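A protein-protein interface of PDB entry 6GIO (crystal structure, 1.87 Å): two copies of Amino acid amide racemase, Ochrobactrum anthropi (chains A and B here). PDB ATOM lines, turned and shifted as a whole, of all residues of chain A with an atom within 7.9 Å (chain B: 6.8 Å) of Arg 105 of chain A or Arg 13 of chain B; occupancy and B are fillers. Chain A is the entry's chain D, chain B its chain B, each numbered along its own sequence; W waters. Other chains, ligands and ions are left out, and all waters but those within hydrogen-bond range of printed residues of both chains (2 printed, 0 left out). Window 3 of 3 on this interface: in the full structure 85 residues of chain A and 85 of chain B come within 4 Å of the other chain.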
ATOM      1  N   VAL A  88     -18.121 -27.989 -21.309  1.00  0.00           N
ATOM      2  CA  VAL A  88     -18.179 -27.183 -20.078  1.00  0.00           C
ATOM      3  C   VAL A  88     -16.778 -27.008 -19.481  1.00  0.00           C
ATOM      4  O   VAL A  88     -16.410 -25.908 -19.094  1.00  0.00           O
ATOM      5  CB  VAL A  88     -19.196 -27.762 -19.078  1.00  0.00           C
ATOM      6  CG1 VAL A  88     -19.223 -26.981 -17.747  1.00  0.00           C
ATOM      7  CG2 VAL A  88     -20.567 -27.723 -19.726  1.00  0.00           C
ATOM      8  N   ALA A  91     -14.823 -24.472 -21.580  1.00  0.00           N
ATOM      9  CA  ALA A  91     -15.249 -23.107 -21.266  1.00  0.00           C
ATOM     10  C   ALA A  91     -14.628 -22.612 -19.951  1.00  0.00           C
ATOM     11  O   ALA A  91     -14.127 -21.444 -19.857  1.00  0.00           O
ATOM     12  CB  ALA A  91     -16.766 -23.016 -21.196  1.00  0.00           C
ATOM     13  N   GLU A  92     -14.639 -23.500 -18.960  1.00  0.00           N
ATOM     14  CA  GLU A  92     -13.967 -23.209 -17.659  1.00  0.00           C
ATOM     15  C   GLU A  92     -12.498 -22.892 -17.884  1.00  0.00           C
ATOM     16  O   GLU A  92     -11.962 -21.936 -17.304  1.00  0.00           O
ATOM     17  CB  GLU A  92     -14.114 -24.383 -16.697  1.00  0.00           C
ATOM     18  CG  GLU A  92     -15.549 -24.568 -16.224  1.00  0.00           C
ATOM     19  CD  GLU A  92     -15.810 -25.835 -15.447  1.00  0.00           C
ATOM     20  OE1 GLU A  92     -15.035 -26.803 -15.561  1.00  0.00           O
ATOM     21  OE2 GLU A  92     -16.828 -25.882 -14.736  1.00  0.00           O
ATOM     22  N   LEU A  95     -12.045 -19.353 -19.631  1.00  0.00           N
ATOM     23  CA  LEU A  95     -12.260 -18.282 -18.641  1.00  0.00           C
ATOM     24  C   LEU A  95     -11.080 -18.180 -17.698  1.00  0.00           C
ATOM     25  O   LEU A  95     -10.613 -17.078 -17.410  1.00  0.00           O
ATOM     26  CB  LEU A  95     -13.556 -18.510 -17.836  1.00  0.00           C
ATOM     27  CG  LEU A  95     -14.846 -18.374 -18.665  1.00  0.00           C
ATOM     28  CD1 LEU A  95     -16.092 -18.784 -17.890  1.00  0.00           C
ATOM     29  CD2 LEU A  95     -15.017 -16.964 -19.194  1.00  0.00           C
ATOM     30  N   GLY A 102     -15.754  -9.304 -14.029  1.00  0.00           N
ATOM     31  CA  GLY A 102     -17.208  -9.496 -14.029  1.00  0.00           C
ATOM     32  C   GLY A 102     -17.614 -10.891 -14.468  1.00  0.00           C
ATOM     33  O   GLY A 102     -16.775 -11.768 -14.536  1.00  0.00           O
ATOM     34  N   GLU A 103     -18.902 -11.067 -14.695  1.00  0.00           N
ATOM     35  CA  GLU A 103     -19.437 -12.353 -15.144  1.00  0.00           C
ATOM     36  C   GLU A 103     -19.183 -12.406 -16.649  1.00  0.00           C
ATOM     37  O   GLU A 103     -19.430 -11.441 -17.310  1.00  0.00           O
ATOM     38  CB  GLU A 103     -20.928 -12.423 -14.831  1.00  0.00           C
ATOM     39  CG  GLU A 103     -21.243 -12.499 -13.354  1.00  0.00           C
ATOM     40  CD  GLU A 103     -21.277 -13.895 -12.760  1.00  0.00           C
ATOM     41  OE1 GLU A 103     -21.103 -14.860 -13.498  1.00  0.00           O
ATOM     42  OE2 GLU A 103     -21.478 -14.003 -11.551  1.00  0.00           O
ATOM     43  N   ARG A 104     -18.646 -13.511 -17.109  1.00  0.00           N
ATOM     44  CA  ARG A 104     -18.393 -13.711 -18.551  1.00  0.00           C
ATOM     45  C   ARG A 104     -18.912 -15.094 -18.937  1.00  0.00           C
ATOM     46  O   ARG A 104     -19.024 -15.914 -18.080  1.00  0.00           O
ATOM     47  CB  ARG A 104     -16.898 -13.644 -18.865  1.00  0.00           C
ATOM     48  CG  ARG A 104     -16.223 -12.349 -18.462  1.00  0.00           C
ATOM     49  CD  ARG A 104     -14.735 -12.378 -18.632  1.00  0.00           C
ATOM     50  NE  ARG A 104     -14.078 -13.304 -17.746  1.00  0.00           N
ATOM     51  CZ  ARG A 104     -12.938 -13.904 -18.037  1.00  0.00           C
ATOM     52  NH1 ARG A 104     -12.386 -13.741 -19.222  1.00  0.00           N
ATOM     53  NH2 ARG A 104     -12.357 -14.676 -17.148  1.00  0.00           N
ATOM     54  N   ARG A 105     -19.211 -15.295 -20.211  1.00  0.00           N
ATOM     55  CA  ARG A 105     -19.616 -16.589 -20.690  1.00  0.00           C
ATOM     56  C   ARG A 105     -18.974 -16.872 -22.049  1.00  0.00           C
ATOM     57  O   ARG A 105     -18.435 -15.965 -22.715  1.00  0.00           O
ATOM     58  CB  ARG A 105     -21.133 -16.672 -20.853  1.00  0.00           C
ATOM     59  CG  ARG A 105     -21.962 -16.390 -19.591  1.00  0.00           C
ATOM     60  CD  ARG A 105     -21.766 -17.458 -18.554  1.00  0.00           C
ATOM     61  NE  ARG A 105     -22.656 -17.321 -17.408  1.00  0.00           N
ATOM     62  CZ  ARG A 105     -22.387 -16.635 -16.291  1.00  0.00           C
ATOM     63  NH1 ARG A 105     -21.289 -15.927 -16.144  1.00  0.00           N
ATOM     64  NH2 ARG A 105     -23.248 -16.669 -15.296  1.00  0.00           N
ATOM     65  N   VAL A 106     -19.114 -18.139 -22.451  1.00  0.00           N
ATOM     66  CA  VAL A 106     -18.459 -18.695 -23.602  1.00  0.00           C
ATOM     67  C   VAL A 106     -19.476 -19.316 -24.540  1.00  0.00           C
ATOM     68  O   VAL A 106     -20.354 -20.119 -24.124  1.00  0.00           O
ATOM     69  CB  VAL A 106     -17.455 -19.803 -23.198  1.00  0.00           C
ATOM     70  CG1 VAL A 106     -16.625 -20.251 -24.409  1.00  0.00           C
ATOM     71  CG2 VAL A 106     -16.563 -19.334 -22.053  1.00  0.00           C
ATOM     72  N   TRP A 107     -19.319 -18.980 -25.805  1.00  0.00           N
ATOM     73  CA  TRP A 107     -20.088 -19.589 -26.872  1.00  0.00           C
ATOM     74  C   TRP A 107     -19.122 -20.373 -27.719  1.00  0.00           C
ATOM     75  O   TRP A 107     -18.012 -19.891 -27.941  1.00  0.00           O
ATOM     76  CB  TRP A 107     -20.697 -18.478 -27.715  1.00  0.00           C
ATOM     77  CG  TRP A 107     -21.355 -18.875 -28.992  1.00  0.00           C
ATOM     78  CD1 TRP A 107     -22.678 -19.130 -29.167  1.00  0.00           C
ATOM     79  CD2 TRP A 107     -20.753 -18.988 -30.292  1.00  0.00           C
ATOM     80  NE1 TRP A 107     -22.934 -19.411 -30.501  1.00  0.00           N
ATOM     81  CE2 TRP A 107     -21.775 -19.342 -31.205  1.00  0.00           C
ATOM     82  CE3 TRP A 107     -19.445 -18.879 -30.766  1.00  0.00           C
ATOM     83  CZ2 TRP A 107     -21.537 -19.539 -32.577  1.00  0.00           C
ATOM     84  CZ3 TRP A 107     -19.206 -19.089 -32.131  1.00  0.00           C
ATOM     85  CH2 TRP A 107     -20.245 -19.425 -33.011  1.00  0.00           C
ATOM     86  N   PHE A 108     -19.530 -21.552 -28.208  1.00  0.00           N
ATOM     87  CA  PHE A 108     -18.677 -22.334 -29.085  1.00  0.00           C
ATOM     88  C   PHE A 108     -19.223 -22.387 -30.504  1.00  0.00           C
ATOM     89  O   PHE A 108     -20.426 -22.384 -30.695  1.00  0.00           O
ATOM     90  CB  PHE A 108     -18.466 -23.747 -28.605  1.00  0.00           C
ATOM     91  CG  PHE A 108     -17.657 -23.845 -27.355  1.00  0.00           C
ATOM     92  CD1 PHE A 108     -16.306 -23.507 -27.351  1.00  0.00           C
ATOM     93  CD2 PHE A 108     -18.260 -24.253 -26.161  1.00  0.00           C
ATOM     94  CE1 PHE A 108     -15.577 -23.589 -26.174  1.00  0.00           C
ATOM     95  CE2 PHE A 108     -17.514 -24.357 -24.990  1.00  0.00           C
ATOM     96  CZ  PHE A 108     -16.188 -24.008 -25.000  1.00  0.00           C
ATOM     97  N   ASP A 261     -13.230  -6.399 -24.154  1.00  0.00           N
ATOM     98  CA  ASP A 261     -14.498  -6.844 -23.639  1.00  0.00           C
ATOM     99  C   ASP A 261     -14.833  -8.255 -24.149  1.00  0.00           C
ATOM    100  O   ASP A 261     -15.439  -9.051 -23.425  1.00  0.00           O
ATOM    101  CB  ASP A 261     -15.589  -5.856 -24.025  1.00  0.00           C
ATOM    102  CG  ASP A 261     -15.352  -4.498 -23.452  1.00  0.00           C
ATOM    103  OD1 ASP A 261     -15.497  -4.389 -22.215  1.00  0.00           O
ATOM    104  OD2 ASP A 261     -15.011  -3.566 -24.213  1.00  0.00           O
ATOM    105  N   MET A 262     -14.387  -8.564 -25.375  1.00  0.00           N
ATOM    106  CA  MET A 262     -14.671  -9.829 -26.004  1.00  0.00           C
ATOM    107  C   MET A 262     -13.441 -10.376 -26.733  1.00  0.00           C
ATOM    108  O   MET A 262     -12.695  -9.627 -27.359  1.00  0.00           O
ATOM    109  CB  MET A 262     -15.828  -9.621 -26.989  1.00  0.00           C
ATOM    110  CG  MET A 262     -16.194 -10.824 -27.839  1.00  0.00           C
ATOM    111  SD  MET A 262     -17.653 -10.538 -28.863  1.00  0.00           S
ATOM    112  CE  MET A 262     -18.910 -10.607 -27.589  1.00  0.00           C
ATOM    113  N   VAL A 263     -13.212 -11.679 -26.619  1.00  0.00           N
ATOM    114  CA  VAL A 263     -12.116 -12.350 -27.340  1.00  0.00           C
ATOM    115  C   VAL A 263     -12.656 -13.447 -28.263  1.00  0.00           C
ATOM    116  O   VAL A 263     -13.528 -14.219 -27.868  1.00  0.00           O
ATOM    117  CB  VAL A 263     -11.049 -12.953 -26.372  1.00  0.00           C
ATOM    118  CG1 VAL A 263      -9.823 -13.397 -27.158  1.00  0.00           C
ATOM    119  CG2 VAL A 263     -10.615 -11.929 -25.323  1.00  0.00           C
ATOM    120  N   ALA A 277     -14.349 -20.185 -30.466  1.00  0.00           N
ATOM    121  CA  ALA A 277     -15.043 -19.699 -29.264  1.00  0.00           C
ATOM    122  C   ALA A 277     -15.106 -18.179 -29.176  1.00  0.00           C
ATOM    123  O   ALA A 277     -14.252 -17.476 -29.689  1.00  0.00           O
ATOM    124  CB  ALA A 277     -14.397 -20.243 -28.011  1.00  0.00           C
ATOM    125  N   VAL A 278     -16.152 -17.696 -28.525  1.00  0.00           N
ATOM    126  CA  VAL A 278     -16.315 -16.300 -28.176  1.00  0.00           C
ATOM    127  C   VAL A 278     -16.464 -16.219 -26.640  1.00  0.00           C
ATOM    128  O   VAL A 278     -17.290 -16.914 -26.030  1.00  0.00           O
ATOM    129  CB  VAL A 278     -17.511 -15.678 -28.898  1.00  0.00           C
ATOM    130  CG1 VAL A 278     -17.711 -14.232 -28.448  1.00  0.00           C
ATOM    131  CG2 VAL A 278     -17.305 -15.710 -30.428  1.00  0.00           C
ATOM    132  N   VAL A 279     -15.606 -15.419 -26.032  1.00  0.00           N
ATOM    133  CA  VAL A 279     -15.662 -15.132 -24.584  1.00  0.00           C
ATOM    134  C   VAL A 279     -16.068 -13.677 -24.468  1.00  0.00           C
ATOM    135  O   VAL A 279     -15.440 -12.813 -25.100  1.00  0.00           O
ATOM    136  CB  VAL A 279     -14.301 -15.333 -23.874  1.00  0.00           C
ATOM    137  CG1 VAL A 279     -14.412 -15.014 -22.384  1.00  0.00           C
ATOM    138  CG2 VAL A 279     -13.813 -16.759 -24.071  1.00  0.00           C
ATOM    139  N   GLY A 280     -17.145 -13.407 -23.738  1.00  0.00           N
ATOM    140  CA  GLY A 280     -17.567 -12.016 -23.526  1.00  0.00           C
ATOM    141  C   GLY A 280     -18.271 -11.826 -22.191  1.00  0.00           C
ATOM    142  O   GLY A 280     -18.437 -12.777 -21.425  1.00  0.00           O
ATOM    143  N   PRO A 281     -18.668 -10.578 -21.898  1.00  0.00           N
ATOM    144  CA  PRO A 281     -19.434 -10.318 -20.670  1.00  0.00           C
ATOM    145  C   PRO A 281     -20.813 -10.994 -20.701  1.00  0.00           C
ATOM    146  O   PRO A 281     -21.425 -11.151 -21.773  1.00  0.00           O
ATOM    147  CB  PRO A 281     -19.535  -8.781 -20.624  1.00  0.00           C
ATOM    148  CG  PRO A 281     -19.215  -8.285 -21.991  1.00  0.00           C
ATOM    149  CD  PRO A 281     -18.646  -9.417 -22.816  1.00  0.00           C
ATOM    150  N   GLN A 282     -21.291 -11.411 -19.531  1.00  0.00           N
ATOM    151  CA  GLN A 282     -22.536 -12.148 -19.432  1.00  0.00           C
ATOM    152  C   GLN A 282     -23.694 -11.318 -20.008  1.00  0.00           C
ATOM    153  O   GLN A 282     -24.561 -11.866 -20.667  1.00  0.00           O
ATOM    154  CB  GLN A 282     -22.855 -12.586 -17.989  1.00  0.00           C
ATOM    155  CG  GLN A 282     -24.291 -13.079 -17.873  1.00  0.00           C
ATOM    156  CD  GLN A 282     -24.674 -13.639 -16.523  1.00  0.00           C
ATOM    157  OE1 GLN A 282     -24.308 -13.084 -15.478  1.00  0.00           O
ATOM    158  NE2 GLN A 282     -25.447 -14.750 -16.532  1.00  0.00           N
ATOM    159  N   TRP A 283     -23.691 -10.006 -19.803  1.00  0.00           N
ATOM    160  CA  TRP A 283     -24.782  -9.195 -20.305  1.00  0.00           C
ATOM    161  C   TRP A 283     -24.933  -9.243 -21.838  1.00  0.00           C
ATOM    162  O   TRP A 283     -26.047  -9.214 -22.346  1.00  0.00           O
ATOM    163  CB  TRP A 283     -24.676  -7.759 -19.801  1.00  0.00           C
ATOM    164  CG  TRP A 283     -23.630  -6.852 -20.363  1.00  0.00           C
ATOM    165  CD1 TRP A 283     -22.425  -6.550 -19.799  1.00  0.00           C
ATOM    166  CD2 TRP A 283     -23.752  -6.006 -21.525  1.00  0.00           C
ATOM    167  NE1 TRP A 283     -21.755  -5.625 -20.581  1.00  0.00           N
ATOM    168  CE2 TRP A 283     -22.548  -5.279 -21.645  1.00  0.00           C
ATOM    169  CE3 TRP A 283     -24.742  -5.840 -22.502  1.00  0.00           C
ATOM    170  CZ2 TRP A 283     -22.309  -4.381 -22.689  1.00  0.00           C
ATOM    171  CZ3 TRP A 283     -24.497  -4.952 -23.566  1.00  0.00           C
ATOM    172  CH2 TRP A 283     -23.297  -4.221 -23.635  1.00  0.00           C
ATOM    173  N   VAL A 284     -23.824  -9.338 -22.568  1.00  0.00           N
ATOM    174  CA  VAL A 284     -23.885  -9.566 -24.039  1.00  0.00           C
ATOM    175  C   VAL A 284     -24.207 -11.004 -24.388  1.00  0.00           C
ATOM    176  O   VAL A 284     -25.060 -11.275 -25.237  1.00  0.00           O
ATOM    177  CB  VAL A 284     -22.550  -9.209 -24.714  1.00  0.00           C
ATOM    178  CG1 VAL A 284     -22.548  -9.598 -26.212  1.00  0.00           C
ATOM    179  CG2 VAL A 284     -22.267  -7.735 -24.534  1.00  0.00           C
ATOM    180  N   MET A 285     -23.482 -11.923 -23.761  1.00  0.00           N
ATOM    181  CA  MET A 285     -23.498 -13.340 -24.153  1.00  0.00           C
ATOM    182  C   MET A 285     -24.794 -14.074 -23.743  1.00  0.00           C
ATOM    183  O   MET A 285     -25.111 -15.154 -24.274  1.00  0.00           O
ATOM    184  CB  MET A 285     -22.246 -14.052 -23.580  1.00  0.00           C
ATOM    185  CG  MET A 285     -20.915 -13.470 -24.039  1.00  0.00           C
ATOM    186  SD  MET A 285     -20.667 -13.462 -25.846  1.00  0.00           S
ATOM    187  CE  MET A 285     -20.712 -15.210 -26.117  1.00  0.00           C
ATOM    188  N   ASP A 286     -25.517 -13.495 -22.776  1.00  0.00           N
ATOM    189  CA  ASP A 286     -26.830 -13.969 -22.395  1.00  0.00           C
ATOM    190  C   ASP A 286     -27.967 -13.096 -22.989  1.00  0.00           C
ATOM    191  O   ASP A 286     -29.063 -13.023 -22.443  1.00  0.00           O
ATOM    192  CB  ASP A 286     -26.912 -14.078 -20.858  1.00  0.00           C
ATOM    193  CG  ASP A 286     -26.122 -15.276 -20.300  1.00  0.00           C
ATOM    194  OD1 ASP A 286     -25.476 -16.021 -21.086  1.00  0.00           O
ATOM    195  OD2 ASP A 286     -26.122 -15.469 -19.058  1.00  0.00           O
ATOM    196  N   LEU B   5     -21.279 -30.095  -7.258  1.00  0.00           N
ATOM    197  CA  LEU B   5     -21.356 -29.108  -8.350  1.00  0.00           C
ATOM    198  C   LEU B   5     -21.674 -29.893  -9.608  1.00  0.00           C
ATOM    199  O   LEU B   5     -20.808 -30.545 -10.198  1.00  0.00           O
ATOM    200  CB  LEU B   5     -20.060 -28.326  -8.529  1.00  0.00           C
ATOM    201  CG  LEU B   5     -20.225 -26.828  -8.842  1.00  0.00           C
ATOM    202  CD1 LEU B   5     -18.974 -26.325  -9.543  1.00  0.00           C
ATOM    203  CD2 LEU B   5     -21.465 -26.473  -9.642  1.00  0.00           C
ATOM    204  N   ARG B   8     -24.722 -29.682 -14.963  1.00  0.00           N
ATOM    205  CA  ARG B   8     -25.765 -28.693 -15.269  1.00  0.00           C
ATOM    206  C   ARG B   8     -25.475 -27.302 -14.673  1.00  0.00           C
ATOM    207  O   ARG B   8     -25.621 -26.273 -15.343  1.00  0.00           O
ATOM    208  CB  ARG B   8     -27.115 -29.190 -14.775  1.00  0.00           C
ATOM    209  CG  ARG B   8     -28.241 -28.225 -15.080  1.00  0.00           C
ATOM    210  CD  ARG B   8     -29.557 -28.830 -14.661  1.00  0.00           C
ATOM    211  NE  ARG B   8     -30.668 -27.972 -15.038  1.00  0.00           N
ATOM    212  CZ  ARG B   8     -31.843 -27.941 -14.422  1.00  0.00           C
ATOM    213  NH1 ARG B   8     -32.080 -28.703 -13.357  1.00  0.00           N
ATOM    214  NH2 ARG B   8     -32.786 -27.117 -14.859  1.00  0.00           N
ATOM    215  N   GLU B   9     -25.029 -27.288 -13.417  1.00  0.00           N
ATOM    216  CA  GLU B   9     -24.736 -26.061 -12.720  1.00  0.00           C
ATOM    217  C   GLU B   9     -23.463 -25.421 -13.255  1.00  0.00           C
ATOM    218  O   GLU B   9     -23.383 -24.229 -13.429  1.00  0.00           O
ATOM    219  CB  GLU B   9     -24.623 -26.324 -11.190  1.00  0.00           C
ATOM    220  CG  GLU B   9     -25.981 -26.564 -10.518  1.00  0.00           C
ATOM    221  CD  GLU B   9     -25.895 -27.018  -9.049  1.00  0.00           C
ATOM    222  OE1 GLU B   9     -25.046 -27.893  -8.684  1.00  0.00           O
ATOM    223  OE2 GLU B   9     -26.698 -26.492  -8.253  1.00  0.00           O
ATOM    224  N   ARG B  10     -22.449 -26.229 -13.498  1.00  0.00           N
ATOM    225  CA  ARG B  10     -21.240 -25.719 -14.103  1.00  0.00           C
ATOM    226  C   ARG B  10     -21.550 -25.081 -15.484  1.00  0.00           C
ATOM    227  O   ARG B  10     -20.975 -24.035 -15.829  1.00  0.00           O
ATOM    228  CB  ARG B  10     -20.218 -26.823 -14.223  1.00  0.00           C
ATOM    229  CG  ARG B  10     -19.539 -27.135 -12.891  1.00  0.00           C
ATOM    230  CD  ARG B  10     -18.822 -28.474 -12.946  1.00  0.00           C
ATOM    231  NE  ARG B  10     -17.802 -28.485 -13.975  1.00  0.00           N
ATOM    232  CZ  ARG B  10     -17.448 -29.558 -14.693  1.00  0.00           C
ATOM    233  NH1 ARG B  10     -18.043 -30.731 -14.494  1.00  0.00           N
ATOM    234  NH2 ARG B  10     -16.491 -29.461 -15.625  1.00  0.00           N
ATOM    235  N   ASP B  11     -22.462 -25.697 -16.227  1.00  0.00           N
ATOM    236  CA  ASP B  11     -22.865 -25.211 -17.554  1.00  0.00           C
ATOM    237  C   ASP B  11     -23.496 -23.840 -17.410  1.00  0.00           C
ATOM    238  O   ASP B  11     -23.209 -22.934 -18.208  1.00  0.00           O
ATOM    239  CB  ASP B  11     -23.817 -26.207 -18.232  1.00  0.00           C
ATOM    240  CG  ASP B  11     -24.348 -25.706 -19.587  1.00  0.00           C
ATOM    241  OD1 ASP B  11     -25.303 -24.900 -19.565  1.00  0.00           O
ATOM    242  OD2 ASP B  11     -23.830 -26.124 -20.660  1.00  0.00           O
ATOM    243  N   ALA B  12     -24.336 -23.673 -16.375  1.00  0.00           N
ATOM    244  CA  ALA B  12     -25.013 -22.392 -16.145  1.00  0.00           C
ATOM    245  C   ALA B  12     -24.053 -21.266 -15.854  1.00  0.00           C
ATOM    246  O   ALA B  12     -24.320 -20.117 -16.237  1.00  0.00           O
ATOM    247  CB  ALA B  12     -26.049 -22.498 -15.022  1.00  0.00           C
ATOM    248  N   ARG B  13     -22.959 -21.573 -15.154  1.00  0.00           N
ATOM    249  CA  ARG B  13     -21.964 -20.572 -14.785  1.00  0.00           C
ATOM    250  C   ARG B  13     -21.103 -20.071 -15.935  1.00  0.00           C
ATOM    251  O   ARG B  13     -20.579 -18.983 -15.843  1.00  0.00           O
ATOM    252  CB  ARG B  13     -21.027 -21.125 -13.718  1.00  0.00           C
ATOM    253  CG  ARG B  13     -21.681 -21.290 -12.356  1.00  0.00           C
ATOM    254  CD  ARG B  13     -20.722 -21.941 -11.369  1.00  0.00           C
ATOM    255  NE  ARG B  13     -21.418 -22.197 -10.111  1.00  0.00           N
ATOM    256  CZ  ARG B  13     -20.856 -22.658  -8.987  1.00  0.00           C
ATOM    257  NH1 ARG B  13     -19.553 -22.946  -8.926  1.00  0.00           N
ATOM    258  NH2 ARG B  13     -21.610 -22.844  -7.912  1.00  0.00           N
ATOM    259  N   VAL B  14     -20.919 -20.859 -17.002  1.00  0.00           N
ATOM    260  CA  VAL B  14     -19.897 -20.519 -18.012  1.00  0.00           C
ATOM    261  C   VAL B  14     -20.361 -20.513 -19.471  1.00  0.00           C
ATOM    262  O   VAL B  14     -19.738 -19.837 -20.307  1.00  0.00           O
ATOM    263  CB  VAL B  14     -18.641 -21.437 -17.875  1.00  0.00           C
ATOM    264  CG1 VAL B  14     -18.108 -21.377 -16.435  1.00  0.00           C
ATOM    265  CG2 VAL B  14     -18.941 -22.862 -18.313  1.00  0.00           C
ATOM    266  N   ILE B  15     -21.450 -21.229 -19.768  1.00  0.00           N
ATOM    267  CA  ILE B  15     -21.969 -21.267 -21.142  1.00  0.00           C
ATOM    268  C   ILE B  15     -22.927 -20.120 -21.479  1.00  0.00           C
ATOM    269  O   ILE B  15     -23.836 -19.800 -20.719  1.00  0.00           O
ATOM    270  CB  ILE B  15     -22.643 -22.616 -21.442  1.00  0.00           C
ATOM    271  CG1 ILE B  15     -21.656 -23.748 -21.178  1.00  0.00           C
ATOM    272  CG2 ILE B  15     -23.128 -22.632 -22.911  1.00  0.00           C
ATOM    273  CD1 ILE B  15     -20.402 -23.683 -22.045  1.00  0.00           C
ATOM    274  N   ALA B  16     -22.730 -19.513 -22.648  1.00  0.00           N
ATOM    275  CA  ALA B  16     -23.566 -18.400 -23.098  1.00  0.00           C
ATOM    276  C   ALA B  16     -25.013 -18.858 -23.381  1.00  0.00           C
ATOM    277  O   ALA B  16     -25.233 -19.833 -24.115  1.00  0.00           O
ATOM    278  CB  ALA B  16     -22.963 -17.772 -24.360  1.00  0.00           C
ATOM    279  N   GLU B  17     -25.987 -18.136 -22.826  1.00  0.00           N
ATOM    280  CA  GLU B  17     -27.409 -18.358 -23.141  1.00  0.00           C
ATOM    281  C   GLU B  17     -27.723 -18.279 -24.647  1.00  0.00           C
ATOM    282  O   GLU B  17     -28.610 -18.946 -25.122  1.00  0.00           O
ATOM    283  CB  GLU B  17     -28.269 -17.311 -22.401  1.00  0.00           C
ATOM    284  CG  GLU B  17     -29.783 -17.501 -22.425  1.00  0.00           C
ATOM    285  CD  GLU B  17     -30.265 -18.746 -21.722  1.00  0.00           C
ATOM    286  OE1 GLU B  17     -29.560 -19.260 -20.819  1.00  0.00           O
ATOM    287  OE2 GLU B  17     -31.360 -19.225 -22.092  1.00  0.00           O
ATOM    288  N   ARG B  20     -27.880 -21.781 -26.234  1.00  0.00           N
ATOM    289  CA  ARG B  20     -28.708 -22.765 -25.586  1.00  0.00           C
ATOM    290  C   ARG B  20     -30.079 -22.928 -26.226  1.00  0.00           C
ATOM    291  O   ARG B  20     -30.709 -21.954 -26.585  1.00  0.00           O
ATOM    292  CB  ARG B  20     -28.963 -22.363 -24.132  1.00  0.00           C
ATOM    293  CG  ARG B  20     -27.784 -22.528 -23.207  1.00  0.00           C
ATOM    294  CD  ARG B  20     -28.298 -22.453 -21.774  1.00  0.00           C
ATOM    295  NE  ARG B  20     -27.196 -22.533 -20.821  1.00  0.00           N
ATOM    296  CZ  ARG B  20     -26.649 -21.501 -20.180  1.00  0.00           C
ATOM    297  NH1 ARG B  20     -27.105 -20.260 -20.326  1.00  0.00           N
ATOM    298  NH2 ARG B  20     -25.624 -21.719 -19.376  1.00  0.00           N
HETATM  299  O   HOH W   1     -18.545 -23.979 -14.283  1.00  0.00           O
HETATM  300  O   HOH W   2     -25.190 -18.173 -19.065  1.00  0.00           O
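The side-chain carboxylate (OE2) of Glu 92 of chain A lies within salt-bridge range of the guanidinium group (NE) of Arg 10 of chain B (2.9 Å). The guanidinium group (NE) of Arg 105 of chain A sits at hydrogen-bond distance from the backbone carbonyl oxygen (O) of Ala 12 of chain B (3.5 Å). The guanidinium group (NE) of Arg 105 of chain A lies close to the backbone carbonyl oxygen (O) of Arg 13 of chain B. N of Val 106 of chain A lies within hydrogen-bond range of O of Val 14 of chain B (2.8 Å). The backbone carbonyl oxygen of Val 106 of chain A lies within hydrogen-bond range of the backbone NH of Ala 16 of chain B (2.9 Å). O of Met 285 of chain A sits at hydrogen-bond distance from N of Glu 17 of chain B. The side-chain carboxylate (OD1) of Asp 286 of chain A is in hydrogen-bond range of the backbone NH (N) of Glu 17 of chain B.
O of Leu 95 of chain A sits at hydrogen-bond distance from NH2 of Arg 104 of chain A. The backbone NH of Arg 105 of chain A lies within hydrogen-bond range of the backbone carbonyl oxygen of Gly 280 of chain A (2.9 Å). OD2 of Asp 286 of chain A is in hydrogen-bond range of NE2 of Gln 282 of chain A. The side-chain carboxylate of Asp 11 of chain B lies within salt-bridge range of the guanidinium group of Arg 20 of chain B, at 3.2 Å. NH2 of Arg 20 of chain B lies within hydrogen-bond range of O of Ile 15 of chain B (2.9 Å). OE1 of Glu 17 of chain B is in salt-bridge range of NH1 of Arg 20 of chain B (2.7 Å).
Among the printed residues, pairs that only touch across the chains: Arg 105 of chain A with Val 14 of chain B (3.3 Å), Met 285 of chain A with Ala 16 of chain B (3.4 Å), Val 106 of chain A with Ile 15 of chain B (3.6 Å), Leu 95 of chain A with Val 14 of chain B (3.6 Å), Ala 91 of chain A with Val 14 of chain B (3.6 Å), Asp 286 of chain A with Ala 16 of chain B (3.7 Å), Val 88 of chain A with Arg 10 of chain B (3.7 Å), Arg 105 of chain A with Ala 16 of chain B (3.7 Å), Val 88 of chain A with Asp 11 of chain B (3.8 Å), Ala 91 of chain A with Ile 15 of chain B (3.8 Å) and Arg 105 of chain A with Ile 15 of chain B (3.8 Å).
Of the printed residues of chain B, Leu 95 of chain A touches Val 14. Of chain B, only Ala 12 (3.5 Å), Arg 13 (3.0 Å), Val 14 (3.3 Å), Ile 15 (3.8 Å) and Ala 16 (3.7 Å) come within 4 Å of Arg 105 of chain A. Printed residues of chain B within 4 Å of Val 106 of chain A: Val 14, Ile 15 and Ala 16. Ala 12 of chain B touches just one residue of chain A: Arg 105 (3.5 Å). Arg 13 of chain B touches just one residue of chain A: Arg 105 (3.0 Å). Of the printed residues of chain A, Val 14 of chain B touches Ala 91 (3.6 Å), Leu 95 (3.6 Å), Arg 105 (3.3 Å) and Val 106 (2.8 Å). Printed residues of chain A within 4 Å of Ile 15 of chain B: Ala 91, Arg 105 and Val 106. The nearest printed residue of chain A that does not touch Glu 17 of chain B is Arg 105 of chain A (5.4 Å).
Of the 24 printed residues of chain A, 8 touch a printed residue of chain B. Among the printed residues, Asp or Glu carboxylates within 4 Å of a Lys or Arg side-chain nitrogen of the other chain: Glu 92 of chain A with Arg 10 of chain B (2.9 Å).
No position is printed for both chains. Of the 18 pairs that touch across the chains among the printed residues, none has its exchanged pair printed and touching as well.
Water W1 bridges OE2 of Glu 92 of chain A (2.6 Å) and O of Arg 10 of chain B (2.9 Å). Water W2 lies within hydrogen-bond range of the backbone carbonyl oxygen of Ile 15 of chain B (2.7 Å), the side-chain carboxylate of Asp 286 of chain A (2.9 Å), the guanidinium group of Arg 20 of chain B (3.1 Å) and the guanidinium group of Arg 105 of chain A (3.1 Å).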
